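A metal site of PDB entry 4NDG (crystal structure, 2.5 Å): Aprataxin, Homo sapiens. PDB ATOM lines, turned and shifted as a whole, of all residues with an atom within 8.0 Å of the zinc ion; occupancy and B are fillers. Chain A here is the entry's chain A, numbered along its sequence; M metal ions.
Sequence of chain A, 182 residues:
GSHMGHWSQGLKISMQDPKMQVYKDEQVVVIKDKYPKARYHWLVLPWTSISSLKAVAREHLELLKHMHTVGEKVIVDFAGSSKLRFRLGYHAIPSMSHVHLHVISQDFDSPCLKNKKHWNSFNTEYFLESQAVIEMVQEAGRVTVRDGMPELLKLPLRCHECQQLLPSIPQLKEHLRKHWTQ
Residues that only touch the zinc ion: Glu 161 (3.96 Å).
The zinc ion is bound by NE2 of His 175 (2.0 Å).
A ring nitrogen (NE2) of His 179 binds the zinc ion, at 2.1 Å.
The zinc ion is bound by the side-chain sulfur (SG) of Cys 162 (2.1 Å).
SG of Cys 159 is bound to the zinc ion (2.4 Å).
The zinc ion has four donor atoms within binding distance.
The backbone NH (N) of Gln 164 lies close to the side-chain sulfur (SG) of Cys 162, at 3.6 Å.
SG of Cys 159 lies close to N of Glu 161 (3.2 Å).
N of Cys 159 lies within hydrogen-bond range of O of Gln 164, at 2.9 Å.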
ATOM      1  N   TRP A 119      14.677  21.471  14.540  1.00  0.00           N
ATOM      2  CA  TRP A 119      14.310  20.080  14.561  1.00  0.00           C
ATOM      3  C   TRP A 119      14.745  19.385  13.280  1.00  0.00           C
ATOM      4  O   TRP A 119      15.330  18.305  13.311  1.00  0.00           O
ATOM      5  CB  TRP A 119      12.807  19.906  14.746  1.00  0.00           C
ATOM      6  CG  TRP A 119      12.442  18.478  14.610  1.00  0.00           C
ATOM      7  CD1 TRP A 119      11.962  17.861  13.502  1.00  0.00           C
ATOM      8  CD2 TRP A 119      12.584  17.468  15.606  1.00  0.00           C
ATOM      9  NE1 TRP A 119      11.776  16.521  13.747  1.00  0.00           N
ATOM     10  CE2 TRP A 119      12.153  16.260  15.029  1.00  0.00           C
ATOM     11  CE3 TRP A 119      13.026  17.464  16.930  1.00  0.00           C
ATOM     12  CZ2 TRP A 119      12.158  15.062  15.738  1.00  0.00           C
ATOM     13  CZ3 TRP A 119      13.022  16.276  17.624  1.00  0.00           C
ATOM     14  CH2 TRP A 119      12.592  15.089  17.035  1.00  0.00           C
ATOM     15  N   ARG A 158       8.218  15.569  12.360  1.00  0.00           N
ATOM     16  CA  ARG A 158       8.058  14.123  12.481  1.00  0.00           C
ATOM     17  C   ARG A 158       8.947  13.592  13.592  1.00  0.00           C
ATOM     18  O   ARG A 158      10.115  13.923  13.669  1.00  0.00           O
ATOM     19  CB  ARG A 158       8.414  13.433  11.168  1.00  0.00           C
ATOM     20  CG  ARG A 158       8.564  11.919  11.297  1.00  0.00           C
ATOM     21  CD  ARG A 158       8.831  11.290   9.941  1.00  0.00           C
ATOM     22  NE  ARG A 158       7.721  11.492   9.011  1.00  0.00           N
ATOM     23  CZ  ARG A 158       6.714  10.648   8.862  1.00  0.00           C
ATOM     24  NH1 ARG A 158       5.746  10.918   7.991  1.00  0.00           N
ATOM     25  NH2 ARG A 158       6.681   9.518   9.558  1.00  0.00           N
ATOM     26  N   CYS A 159       8.368  12.781  14.471  1.00  0.00           N
ATOM     27  CA  CYS A 159       9.106  12.219  15.593  1.00  0.00           C
ATOM     28  C   CYS A 159      10.216  11.263  15.140  1.00  0.00           C
ATOM     29  O   CYS A 159      10.001  10.407  14.296  1.00  0.00           O
ATOM     30  CB  CYS A 159       8.165  11.484  16.549  1.00  0.00           C
ATOM     31  SG  CYS A 159       8.974  10.881  18.067  1.00  0.00           S
ATOM     32  N   HIS A 160      11.408  11.421  15.708  1.00  0.00           N
ATOM     33  CA  HIS A 160      12.529  10.554  15.374  1.00  0.00           C
ATOM     34  C   HIS A 160      12.415   9.197  16.070  1.00  0.00           C
ATOM     35  O   HIS A 160      13.171   8.280  15.784  1.00  0.00           O
ATOM     36  CB  HIS A 160      13.856  11.219  15.742  1.00  0.00           C
ATOM     37  CG  HIS A 160      14.079  11.300  17.217  1.00  0.00           C
ATOM     38  ND1 HIS A 160      13.198  11.931  18.069  1.00  0.00           N
ATOM     39  CD2 HIS A 160      15.095  10.844  17.992  1.00  0.00           C
ATOM     40  CE1 HIS A 160      13.658  11.844  19.302  1.00  0.00           C
ATOM     41  NE2 HIS A 160      14.806  11.198  19.284  1.00  0.00           N
ATOM     42  N   GLU A 161      11.443   9.088  16.970  1.00  0.00           N
ATOM     43  CA  GLU A 161      11.240   7.889  17.779  1.00  0.00           C
ATOM     44  C   GLU A 161      10.100   7.020  17.252  1.00  0.00           C
ATOM     45  O   GLU A 161      10.316   5.854  16.929  1.00  0.00           O
ATOM     46  CB  GLU A 161      10.961   8.264  19.251  1.00  0.00           C
ATOM     47  CG  GLU A 161      12.137   8.866  20.057  1.00  0.00           C
ATOM     48  CD  GLU A 161      13.075   7.797  20.614  1.00  0.00           C
ATOM     49  OE1 GLU A 161      12.666   6.617  20.679  1.00  0.00           O
ATOM     50  OE2 GLU A 161      14.213   8.146  21.010  1.00  0.00           O
ATOM     51  N   CYS A 162       8.882   7.558  17.224  1.00  0.00           N
ATOM     52  CA  CYS A 162       7.742   6.800  16.731  1.00  0.00           C
ATOM     53  C   CYS A 162       7.353   7.069  15.262  1.00  0.00           C
ATOM     54  O   CYS A 162       6.440   6.427  14.733  1.00  0.00           O
ATOM     55  CB  CYS A 162       6.534   7.066  17.612  1.00  0.00           C
ATOM     56  SG  CYS A 162       5.988   8.756  17.554  1.00  0.00           S
ATOM     57  N   GLN A 163       8.024   8.032  14.631  1.00  0.00           N
ATOM     58  CA  GLN A 163       7.841   8.368  13.212  1.00  0.00           C
ATOM     59  C   GLN A 163       6.465   8.962  12.966  1.00  0.00           C
ATOM     60  O   GLN A 163       5.966   8.951  11.848  1.00  0.00           O
ATOM     61  CB  GLN A 163       8.023   7.128  12.331  1.00  0.00           C
ATOM     62  CG  GLN A 163       8.934   7.232  11.118  1.00  0.00           C
ATOM     63  CD  GLN A 163      10.291   7.814  11.468  1.00  0.00           C
ATOM     64  OE1 GLN A 163      10.926   7.384  12.443  1.00  0.00           O
ATOM     65  NE2 GLN A 163      10.798   8.709  10.619  1.00  0.00           N
ATOM     66  N   GLN A 164       5.861   9.516  14.009  1.00  0.00           N
ATOM     67  CA  GLN A 164       4.511  10.053  13.882  1.00  0.00           C
ATOM     68  C   GLN A 164       4.617  11.509  13.480  1.00  0.00           C
ATOM     69  O   GLN A 164       5.590  12.186  13.827  1.00  0.00           O
ATOM     70  CB  GLN A 164       3.725   9.932  15.185  1.00  0.00           C
ATOM     71  CG  GLN A 164       2.287  10.430  15.120  1.00  0.00           C
ATOM     72  CD  GLN A 164       1.713  10.692  16.495  1.00  0.00           C
ATOM     73  OE1 GLN A 164       2.026  10.005  17.451  1.00  0.00           O
ATOM     74  NE2 GLN A 164       0.848  11.702  16.584  1.00  0.00           N
ATOM     75  N   LEU A 165       3.649  11.998  12.714  1.00  0.00           N
ATOM     76  CA  LEU A 165       3.628  13.391  12.302  1.00  0.00           C
ATOM     77  C   LEU A 165       3.111  14.285  13.429  1.00  0.00           C
ATOM     78  O   LEU A 165       2.194  13.922  14.157  1.00  0.00           O
ATOM     79  CB  LEU A 165       2.750  13.536  11.060  1.00  0.00           C
ATOM     80  CG  LEU A 165       2.686  14.918  10.414  1.00  0.00           C
ATOM     81  CD1 LEU A 165       4.057  15.313   9.918  1.00  0.00           C
ATOM     82  CD2 LEU A 165       1.675  14.947   9.287  1.00  0.00           C
ATOM     83  N   LEU A 166       3.724  15.459  13.605  1.00  0.00           N
ATOM     84  CA  LEU A 166       3.250  16.451  14.563  1.00  0.00           C
ATOM     85  C   LEU A 166       3.047  17.798  13.864  1.00  0.00           C
ATOM     86  O   LEU A 166       3.796  18.135  12.947  1.00  0.00           O
ATOM     87  CB  LEU A 166       4.211  16.601  15.742  1.00  0.00           C
ATOM     88  CG  LEU A 166       4.142  15.589  16.892  1.00  0.00           C
ATOM     89  CD1 LEU A 166       2.706  15.411  17.369  1.00  0.00           C
ATOM     90  CD2 LEU A 166       4.753  14.255  16.504  1.00  0.00           C
ATOM     91  N   LEU A 172       5.043  18.753  19.441  1.00  0.00           N
ATOM     92  CA  LEU A 172       6.127  17.809  19.248  1.00  0.00           C
ATOM     93  C   LEU A 172       6.859  17.584  20.569  1.00  0.00           C
ATOM     94  O   LEU A 172       7.198  16.464  20.908  1.00  0.00           O
ATOM     95  CB  LEU A 172       7.095  18.304  18.183  1.00  0.00           C
ATOM     96  CG  LEU A 172       8.320  17.419  17.938  1.00  0.00           C
ATOM     97  CD1 LEU A 172       7.885  16.000  17.608  1.00  0.00           C
ATOM     98  CD2 LEU A 172       9.190  17.992  16.821  1.00  0.00           C
ATOM     99  N   HIS A 175       4.804  15.619  22.871  1.00  0.00           N
ATOM    100  CA  HIS A 175       4.873  14.232  22.429  1.00  0.00           C
ATOM    101  C   HIS A 175       6.163  13.544  22.885  1.00  0.00           C
ATOM    102  O   HIS A 175       6.138  12.405  23.333  1.00  0.00           O
ATOM    103  CB  HIS A 175       4.755  14.161  20.916  1.00  0.00           C
ATOM    104  CG  HIS A 175       5.037  12.812  20.356  1.00  0.00           C
ATOM    105  ND1 HIS A 175       4.039  11.888  20.096  1.00  0.00           N
ATOM    106  CD2 HIS A 175       6.198  12.204  20.025  1.00  0.00           C
ATOM    107  CE1 HIS A 175       4.581  10.783  19.620  1.00  0.00           C
ATOM    108  NE2 HIS A 175       5.888  10.949  19.563  1.00  0.00           N
ATOM    109  N   LEU A 176       7.287  14.248  22.758  1.00  0.00           N
ATOM    110  CA  LEU A 176       8.583  13.686  23.123  1.00  0.00           C
ATOM    111  C   LEU A 176       8.682  13.413  24.617  1.00  0.00           C
ATOM    112  O   LEU A 176       9.326  12.452  25.025  1.00  0.00           O
ATOM    113  CB  LEU A 176       9.721  14.613  22.699  1.00  0.00           C
ATOM    114  CG  LEU A 176      10.060  14.651  21.204  1.00  0.00           C
ATOM    115  CD1 LEU A 176      11.223  15.588  20.959  1.00  0.00           C
ATOM    116  CD2 LEU A 176      10.351  13.263  20.666  1.00  0.00           C
ATOM    117  N   ARG A 177       8.040  14.267  25.405  1.00  0.00           N
ATOM    118  CA  ARG A 177       8.008  14.115  26.853  1.00  0.00           C
ATOM    119  C   ARG A 177       7.762  12.686  27.322  1.00  0.00           C
ATOM    120  O   ARG A 177       8.334  12.235  28.320  1.00  0.00           O
ATOM    121  CB  ARG A 177       6.915  15.005  27.452  1.00  0.00           C
ATOM    122  CG  ARG A 177       7.339  16.421  27.785  1.00  0.00           C
ATOM    123  CD  ARG A 177       6.123  17.272  28.148  1.00  0.00           C
ATOM    124  NE  ARG A 177       5.303  16.661  29.186  1.00  0.00           N
ATOM    125  CZ  ARG A 177       5.246  17.081  30.446  1.00  0.00           C
ATOM    126  NH1 ARG A 177       5.967  18.120  30.842  1.00  0.00           N
ATOM    127  NH2 ARG A 177       4.463  16.461  31.326  1.00  0.00           N
ATOM    128  N   LYS A 178       6.913  11.970  26.592  1.00  0.00           N
ATOM    129  CA  LYS A 178       6.460  10.657  27.014  1.00  0.00           C
ATOM    130  C   LYS A 178       7.425   9.552  26.583  1.00  0.00           C
ATOM    131  O   LYS A 178       7.397   8.439  27.115  1.00  0.00           O
ATOM    132  CB  LYS A 178       5.058  10.447  26.461  1.00  0.00           C
ATOM    133  CG  LYS A 178       4.100  11.427  27.123  1.00  0.00           C
ATOM    134  CD  LYS A 178       2.806  11.622  26.356  1.00  0.00           C
ATOM    135  CE  LYS A 178       1.910  12.606  27.105  1.00  0.00           C
ATOM    136  NZ  LYS A 178       0.690  12.980  26.336  1.00  0.00           N
ATOM    137  N   HIS A 179       8.290   9.865  25.626  1.00  0.00           N
ATOM    138  CA  HIS A 179       9.309   8.922  25.179  1.00  0.00           C
ATOM    139  C   HIS A 179      10.453   8.852  26.204  1.00  0.00           C
ATOM    140  O   HIS A 179      11.267   7.935  26.151  1.00  0.00           O
ATOM    141  CB  HIS A 179       9.870   9.324  23.802  1.00  0.00           C
ATOM    142  CG  HIS A 179       9.030   8.870  22.631  1.00  0.00           C
ATOM    143  ND1 HIS A 179       8.792   7.544  22.347  1.00  0.00           N
ATOM    144  CD2 HIS A 179       8.408   9.579  21.662  1.00  0.00           C
ATOM    145  CE1 HIS A 179       8.051   7.457  21.259  1.00  0.00           C
ATOM    146  NE2 HIS A 179       7.800   8.678  20.820  1.00  0.00           N
HETATM  147 ZN    ZN M   1       7.222   9.565  19.046  1.00  0.00          ZN
